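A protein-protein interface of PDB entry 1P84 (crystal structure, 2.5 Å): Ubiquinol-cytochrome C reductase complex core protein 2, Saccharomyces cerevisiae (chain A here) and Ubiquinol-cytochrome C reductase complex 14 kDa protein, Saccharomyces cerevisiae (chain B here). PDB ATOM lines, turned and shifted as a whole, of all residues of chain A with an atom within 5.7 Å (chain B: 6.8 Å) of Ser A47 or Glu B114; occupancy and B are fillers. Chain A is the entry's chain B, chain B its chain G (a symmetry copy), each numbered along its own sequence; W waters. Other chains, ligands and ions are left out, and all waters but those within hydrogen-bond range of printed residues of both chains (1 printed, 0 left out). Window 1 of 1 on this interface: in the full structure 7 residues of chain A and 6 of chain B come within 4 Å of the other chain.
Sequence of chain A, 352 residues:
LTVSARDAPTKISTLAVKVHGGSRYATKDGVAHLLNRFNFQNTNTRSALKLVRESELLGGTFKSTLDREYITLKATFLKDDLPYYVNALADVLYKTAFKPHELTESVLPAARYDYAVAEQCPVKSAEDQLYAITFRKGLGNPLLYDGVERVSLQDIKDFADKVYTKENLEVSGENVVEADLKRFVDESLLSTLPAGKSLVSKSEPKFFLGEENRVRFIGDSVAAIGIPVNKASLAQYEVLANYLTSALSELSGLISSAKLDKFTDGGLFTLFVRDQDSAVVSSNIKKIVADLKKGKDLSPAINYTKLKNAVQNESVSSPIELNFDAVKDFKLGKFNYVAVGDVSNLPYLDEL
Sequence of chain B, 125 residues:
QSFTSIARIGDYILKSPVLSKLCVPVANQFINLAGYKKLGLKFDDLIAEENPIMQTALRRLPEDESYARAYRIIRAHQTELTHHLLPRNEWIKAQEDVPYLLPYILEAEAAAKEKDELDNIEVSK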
ATOM      1  N   GLN A  41     -19.804  -6.960 -19.742  1.00  0.00           N
ATOM      2  CA  GLN A  41     -18.973  -6.472 -20.833  1.00  0.00           C
ATOM      3  C   GLN A  41     -19.144  -4.944 -20.791  1.00  0.00           C
ATOM      4  O   GLN A  41     -19.168  -4.344 -19.707  1.00  0.00           O
ATOM      5  CB  GLN A  41     -19.450  -7.022 -22.180  1.00  0.00           C
ATOM      6  CG  GLN A  41     -18.907  -8.395 -22.524  1.00  0.00           C
ATOM      7  CD  GLN A  41     -17.390  -8.409 -22.680  1.00  0.00           C
ATOM      8  OE1 GLN A  41     -16.707  -9.256 -22.106  1.00  0.00           O
ATOM      9  NE2 GLN A  41     -16.860  -7.476 -23.465  1.00  0.00           N
ATOM     10  N   ASN A  42     -19.310  -4.312 -21.947  1.00  0.00           N
ATOM     11  CA  ASN A  42     -19.473  -2.861 -21.971  1.00  0.00           C
ATOM     12  C   ASN A  42     -20.906  -2.363 -21.878  1.00  0.00           C
ATOM     13  O   ASN A  42     -21.805  -2.924 -22.500  1.00  0.00           O
ATOM     14  CB  ASN A  42     -18.837  -2.262 -23.229  1.00  0.00           C
ATOM     15  CG  ASN A  42     -17.377  -1.931 -23.046  1.00  0.00           C
ATOM     16  OD1 ASN A  42     -16.854  -1.955 -21.933  1.00  0.00           O
ATOM     17  ND2 ASN A  42     -16.709  -1.608 -24.140  1.00  0.00           N
ATOM     18  N   THR A  43     -21.111  -1.339 -21.051  1.00  0.00           N
ATOM     19  CA  THR A  43     -22.418  -0.696 -20.924  1.00  0.00           C
ATOM     20  C   THR A  43     -22.233   0.603 -21.710  1.00  0.00           C
ATOM     21  O   THR A  43     -21.130   0.889 -22.175  1.00  0.00           O
ATOM     22  CB  THR A  43     -22.810  -0.339 -19.456  1.00  0.00           C
ATOM     23  OG1 THR A  43     -21.956   0.699 -18.960  1.00  0.00           O
ATOM     24  CG2 THR A  43     -22.729  -1.555 -18.553  1.00  0.00           C
ATOM     25  N   THR A  45     -22.231   3.599 -20.553  1.00  0.00           N
ATOM     26  CA  THR A  45     -21.571   4.638 -19.764  1.00  0.00           C
ATOM     27  C   THR A  45     -20.296   4.171 -19.050  1.00  0.00           C
ATOM     28  O   THR A  45     -19.454   4.990 -18.651  1.00  0.00           O
ATOM     29  CB  THR A  45     -22.533   5.240 -18.694  1.00  0.00           C
ATOM     30  OG1 THR A  45     -22.926   4.225 -17.756  1.00  0.00           O
ATOM     31  CG2 THR A  45     -23.773   5.831 -19.362  1.00  0.00           C
ATOM     32  N   ARG A  46     -20.158   2.856 -18.900  1.00  0.00           N
ATOM     33  CA  ARG A  46     -19.014   2.275 -18.208  1.00  0.00           C
ATOM     34  C   ARG A  46     -18.440   1.132 -19.034  1.00  0.00           C
ATOM     35  O   ARG A  46     -19.185   0.305 -19.565  1.00  0.00           O
ATOM     36  CB  ARG A  46     -19.474   1.735 -16.850  1.00  0.00           C
ATOM     37  CG  ARG A  46     -18.398   1.630 -15.786  1.00  0.00           C
ATOM     38  CD  ARG A  46     -18.648   2.635 -14.661  1.00  0.00           C
ATOM     39  NE  ARG A  46     -19.190   2.056 -13.420  1.00  0.00           N
ATOM     40  CZ  ARG A  46     -20.389   1.486 -13.280  1.00  0.00           C
ATOM     41  NH1 ARG A  46     -20.751   1.016 -12.097  1.00  0.00           N
ATOM     42  NH2 ARG A  46     -21.219   1.350 -14.309  1.00  0.00           N
ATOM     43  N   SER A  47     -17.117   1.098 -19.162  1.00  0.00           N
ATOM     44  CA  SER A  47     -16.451   0.024 -19.906  1.00  0.00           C
ATOM     45  C   SER A  47     -16.167  -1.126 -18.943  1.00  0.00           C
ATOM     46  O   SER A  47     -16.045  -0.912 -17.726  1.00  0.00           O
ATOM     47  CB  SER A  47     -15.132   0.505 -20.518  1.00  0.00           C
ATOM     48  OG  SER A  47     -14.152   0.727 -19.514  1.00  0.00           O
ATOM     49  N   ALA A  48     -16.063  -2.337 -19.486  1.00  0.00           N
ATOM     50  CA  ALA A  48     -15.778  -3.527 -18.681  1.00  0.00           C
ATOM     51  C   ALA A  48     -14.496  -3.321 -17.857  1.00  0.00           C
ATOM     52  O   ALA A  48     -14.381  -3.791 -16.724  1.00  0.00           O
ATOM     53  CB  ALA A  48     -15.644  -4.742 -19.581  1.00  0.00           C
ATOM     54  N   LEU A  49     -13.562  -2.568 -18.427  1.00  0.00           N
ATOM     55  CA  LEU A  49     -12.300  -2.262 -17.776  1.00  0.00           C
ATOM     56  C   LEU A  49     -12.487  -1.340 -16.565  1.00  0.00           C
ATOM     57  O   LEU A  49     -11.975  -1.629 -15.479  1.00  0.00           O
ATOM     58  CB  LEU A  49     -11.328  -1.638 -18.795  1.00  0.00           C
ATOM     59  CG  LEU A  49      -9.993  -1.039 -18.337  1.00  0.00           C
ATOM     60  CD1 LEU A  49      -9.104  -2.084 -17.704  1.00  0.00           C
ATOM     61  CD2 LEU A  49      -9.317  -0.418 -19.530  1.00  0.00           C
ATOM     62  N   LYS A  50     -13.212  -0.236 -16.751  1.00  0.00           N
ATOM     63  CA  LYS A  50     -13.449   0.713 -15.658  1.00  0.00           C
ATOM     64  C   LYS A  50     -14.230   0.055 -14.518  1.00  0.00           C
ATOM     65  O   LYS A  50     -13.934   0.266 -13.330  1.00  0.00           O
ATOM     66  CB  LYS A  50     -14.186   1.965 -16.152  1.00  0.00           C
ATOM     67  CG  LYS A  50     -14.206   3.086 -15.111  1.00  0.00           C
ATOM     68  CD  LYS A  50     -14.541   4.432 -15.726  1.00  0.00           C
ATOM     69  CE  LYS A  50     -14.310   5.563 -14.718  1.00  0.00           C
ATOM     70  NZ  LYS A  50     -14.478   6.928 -15.321  1.00  0.00           N
ATOM     71  N   LEU A  51     -15.201  -0.773 -14.896  1.00  0.00           N
ATOM     72  CA  LEU A  51     -16.018  -1.485 -13.932  1.00  0.00           C
ATOM     73  C   LEU A  51     -15.139  -2.314 -13.000  1.00  0.00           C
ATOM     74  O   LEU A  51     -15.271  -2.236 -11.776  1.00  0.00           O
ATOM     75  CB  LEU A  51     -17.016  -2.390 -14.660  1.00  0.00           C
ATOM     76  CG  LEU A  51     -18.007  -3.183 -13.806  1.00  0.00           C
ATOM     77  CD1 LEU A  51     -18.730  -2.235 -12.859  1.00  0.00           C
ATOM     78  CD2 LEU A  51     -18.999  -3.899 -14.719  1.00  0.00           C
ATOM     79  N   VAL A  52     -14.216  -3.076 -13.585  1.00  0.00           N
ATOM     80  CA  VAL A  52     -13.319  -3.921 -12.813  1.00  0.00           C
ATOM     81  C   VAL A  52     -12.331  -3.110 -11.976  1.00  0.00           C
ATOM     82  O   VAL A  52     -12.139  -3.375 -10.789  1.00  0.00           O
ATOM     83  CB  VAL A  52     -12.532  -4.904 -13.726  1.00  0.00           C
ATOM     84  CG1 VAL A  52     -11.601  -5.769 -12.894  1.00  0.00           C
ATOM     85  CG2 VAL A  52     -13.482  -5.774 -14.535  1.00  0.00           C
ATOM     86  N   GLU B 109      -8.600   4.595 -29.720  1.00  0.00           N
ATOM     87  CA  GLU B 109      -7.812   5.605 -29.009  1.00  0.00           C
ATOM     88  C   GLU B 109      -8.370   5.925 -27.623  1.00  0.00           C
ATOM     89  O   GLU B 109      -7.611   6.117 -26.668  1.00  0.00           O
ATOM     90  CB  GLU B 109      -7.683   6.892 -29.828  1.00  0.00           C
ATOM     91  CG  GLU B 109      -6.702   6.800 -30.982  1.00  0.00           C
ATOM     92  CD  GLU B 109      -6.527   8.113 -31.726  1.00  0.00           C
ATOM     93  OE1 GLU B 109      -6.074   8.082 -32.889  1.00  0.00           O
ATOM     94  OE2 GLU B 109      -6.829   9.178 -31.159  1.00  0.00           O
ATOM     95  N   ALA B 110      -9.698   5.978 -27.515  1.00  0.00           N
ATOM     96  CA  ALA B 110     -10.355   6.265 -26.236  1.00  0.00           C
ATOM     97  C   ALA B 110     -10.121   5.100 -25.273  1.00  0.00           C
ATOM     98  O   ALA B 110      -9.791   5.303 -24.093  1.00  0.00           O
ATOM     99  CB  ALA B 110     -11.844   6.496 -26.450  1.00  0.00           C
ATOM    100  N   ALA B 111     -10.274   3.879 -25.794  1.00  0.00           N
ATOM    101  CA  ALA B 111     -10.055   2.662 -25.012  1.00  0.00           C
ATOM    102  C   ALA B 111      -8.617   2.665 -24.492  1.00  0.00           C
ATOM    103  O   ALA B 111      -8.376   2.431 -23.300  1.00  0.00           O
ATOM    104  CB  ALA B 111     -10.299   1.439 -25.871  1.00  0.00           C
ATOM    105  N   ALA B 112      -7.680   2.986 -25.384  1.00  0.00           N
ATOM    106  CA  ALA B 112      -6.262   3.048 -25.046  1.00  0.00           C
ATOM    107  C   ALA B 112      -5.970   4.117 -23.991  1.00  0.00           C
ATOM    108  O   ALA B 112      -5.272   3.853 -23.008  1.00  0.00           O
ATOM    109  CB  ALA B 112      -5.438   3.311 -26.303  1.00  0.00           C
ATOM    110  N   LYS B 113      -6.502   5.323 -24.213  1.00  0.00           N
ATOM    111  CA  LYS B 113      -6.327   6.445 -23.293  1.00  0.00           C
ATOM    112  C   LYS B 113      -6.901   6.117 -21.905  1.00  0.00           C
ATOM    113  O   LYS B 113      -6.289   6.431 -20.882  1.00  0.00           O
ATOM    114  CB  LYS B 113      -6.984   7.706 -23.868  1.00  0.00           C
ATOM    115  CG  LYS B 113      -6.903   8.934 -22.959  1.00  0.00           C
ATOM    116  CD  LYS B 113      -5.453   9.331 -22.644  1.00  0.00           C
ATOM    117  CE  LYS B 113      -4.813  10.139 -23.778  1.00  0.00           C
ATOM    118  NZ  LYS B 113      -5.458  11.483 -23.932  1.00  0.00           N
ATOM    119  N   GLU B 114      -8.060   5.459 -21.868  1.00  0.00           N
ATOM    120  CA  GLU B 114      -8.659   5.088 -20.591  1.00  0.00           C
ATOM    121  C   GLU B 114      -7.708   4.169 -19.825  1.00  0.00           C
ATOM    122  O   GLU B 114      -7.411   4.413 -18.648  1.00  0.00           O
ATOM    123  CB  GLU B 114     -10.017   4.404 -20.784  1.00  0.00           C
ATOM    124  CG  GLU B 114     -10.706   4.035 -19.462  1.00  0.00           C
ATOM    125  CD  GLU B 114     -12.126   3.529 -19.648  1.00  0.00           C
ATOM    126  OE1 GLU B 114     -12.354   2.658 -20.513  1.00  0.00           O
ATOM    127  OE2 GLU B 114     -13.021   4.013 -18.925  1.00  0.00           O
ATOM    128  N   LYS B 115      -7.198   3.139 -20.503  1.00  0.00           N
ATOM    129  CA  LYS B 115      -6.273   2.219 -19.859  1.00  0.00           C
ATOM    130  C   LYS B 115      -5.055   2.957 -19.326  1.00  0.00           C
ATOM    131  O   LYS B 115      -4.589   2.686 -18.224  1.00  0.00           O
ATOM    132  CB  LYS B 115      -5.820   1.109 -20.802  1.00  0.00           C
ATOM    133  CG  LYS B 115      -4.978   0.060 -20.080  1.00  0.00           C
ATOM    134  CD  LYS B 115      -4.347  -0.947 -21.022  1.00  0.00           C
ATOM    135  CE  LYS B 115      -3.791  -2.138 -20.250  1.00  0.00           C
ATOM    136  NZ  LYS B 115      -2.807  -1.724 -19.215  1.00  0.00           N
ATOM    137  N   ASP B 116      -4.551   3.910 -20.097  1.00  0.00           N
ATOM    138  CA  ASP B 116      -3.389   4.663 -19.653  1.00  0.00           C
ATOM    139  C   ASP B 116      -3.756   5.423 -18.374  1.00  0.00           C
ATOM    140  O   ASP B 116      -2.988   5.429 -17.411  1.00  0.00           O
ATOM    141  CB  ASP B 116      -2.904   5.613 -20.752  1.00  0.00           C
ATOM    142  CG  ASP B 116      -1.537   6.225 -20.441  1.00  0.00           C
ATOM    143  OD1 ASP B 116      -0.590   5.453 -20.161  1.00  0.00           O
ATOM    144  OD2 ASP B 116      -1.402   7.473 -20.472  1.00  0.00           O
ATOM    145  N   GLU B 117      -4.961   5.997 -18.355  1.00  0.00           N
ATOM    146  CA  GLU B 117      -5.467   6.754 -17.206  1.00  0.00           C
ATOM    147  C   GLU B 117      -5.633   5.880 -15.972  1.00  0.00           C
ATOM    148  O   GLU B 117      -5.152   6.224 -14.889  1.00  0.00           O
ATOM    149  CB  GLU B 117      -6.804   7.418 -17.550  1.00  0.00           C
ATOM    150  CG  GLU B 117      -6.693   8.885 -17.954  1.00  0.00           C
ATOM    151  CD  GLU B 117      -7.727   9.311 -18.999  1.00  0.00           C
ATOM    152  OE1 GLU B 117      -8.789   8.657 -19.138  1.00  0.00           O
ATOM    153  OE2 GLU B 117      -7.464  10.309 -19.706  1.00  0.00           O
ATOM    154  N   LEU B 118      -6.300   4.744 -16.147  1.00  0.00           N
ATOM    155  CA  LEU B 118      -6.531   3.812 -15.052  1.00  0.00           C
ATOM    156  C   LEU B 118      -5.264   3.161 -14.467  1.00  0.00           C
ATOM    157  O   LEU B 118      -5.194   2.934 -13.253  1.00  0.00           O
ATOM    158  CB  LEU B 118      -7.544   2.748 -15.478  1.00  0.00           C
ATOM    159  CG  LEU B 118      -8.952   3.304 -15.718  1.00  0.00           C
ATOM    160  CD1 LEU B 118      -9.866   2.220 -16.254  1.00  0.00           C
ATOM    161  CD2 LEU B 118      -9.514   3.885 -14.431  1.00  0.00           C
ATOM    162  N   ASP B 119      -4.271   2.862 -15.307  1.00  0.00           N
ATOM    163  CA  ASP B 119      -3.023   2.254 -14.823  1.00  0.00           C
ATOM    164  C   ASP B 119      -2.230   3.229 -13.950  1.00  0.00           C
ATOM    165  O   ASP B 119      -1.372   2.810 -13.167  1.00  0.00           O
ATOM    166  CB  ASP B 119      -2.120   1.821 -15.987  1.00  0.00           C
ATOM    167  CG  ASP B 119      -2.685   0.661 -16.788  1.00  0.00           C
ATOM    168  OD1 ASP B 119      -3.530  -0.090 -16.268  1.00  0.00           O
ATOM    169  OD2 ASP B 119      -2.271   0.497 -17.956  1.00  0.00           O
ATOM    170  N   ASN B 120      -2.521   4.523 -14.093  1.00  0.00           N
ATOM    171  CA  ASN B 120      -1.813   5.559 -13.351  1.00  0.00           C
ATOM    172  C   ASN B 120      -2.624   6.368 -12.342  1.00  0.00           C
ATOM    173  O   ASN B 120      -2.121   7.364 -11.815  1.00  0.00           O
ATOM    174  CB  ASN B 120      -1.127   6.526 -14.321  1.00  0.00           C
ATOM    175  CG  ASN B 120      -0.038   5.865 -15.130  1.00  0.00           C
ATOM    176  OD1 ASN B 120       0.993   5.467 -14.595  1.00  0.00           O
ATOM    177  ND2 ASN B 120      -0.265   5.740 -16.431  1.00  0.00           N
HETATM  178  O   HOH W   1     -15.798   3.816 -19.239  1.00  0.00           O
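OE1 of Glu B114 is in hydrogen-bond range of OG of Ser A47, at 2.8 Å.
OG of Ser A47 sits at hydrogen-bond distance from N of Lys A50 (3.1 Å).
Among the printed residues, pairs that only touch across the chains: Leu A49 with Leu B118, Lys A50 with Glu B114 and Lys A50 with Leu B118.
Thr A43 touches none of the printed residues of chain B. Of the printed residues of chain B, Ser A47 touches Glu B114. Of the printed residues of chain B, Lys A50 touches Glu B114 (3.6 Å) and Leu B118 (3.9 Å). Glu B117 touches none of the printed residues of chain A. Of the printed residues of chain A, Leu B118 touches Leu A49 and Lys A50. The nearest residue of chain B that does not touch Ser A47 is Leu B118 (5.6 Å). The nearest residue of chain A that does not touch Glu B114 is Leu A49 (4.4 Å).
Printed residues of chain B that touch a printed residue of chain A: Glu B114 and Leu B118. Hydrophobic or aromatic side chains of chain B that line the printed part of chain A: Leu B118. Of the 11 printed residues of chain A, 3 touch a printed residue of chain B. Printed residues of chain A that touch a printed residue of chain B: Ser A47, Leu A49 and Lys A50. Hydrophobic or aromatic side chains of chain A that line the printed part of chain B: Leu A49. Among the printed residues, no Asp or Glu carboxylate lies within 4 Å of a Lys or Arg side-chain nitrogen of the other chain.
Water W1 lies within hydrogen-bond range of OE2 of Glu B114 (2.8 Å) and N of Ser A47 (3.0 Å).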
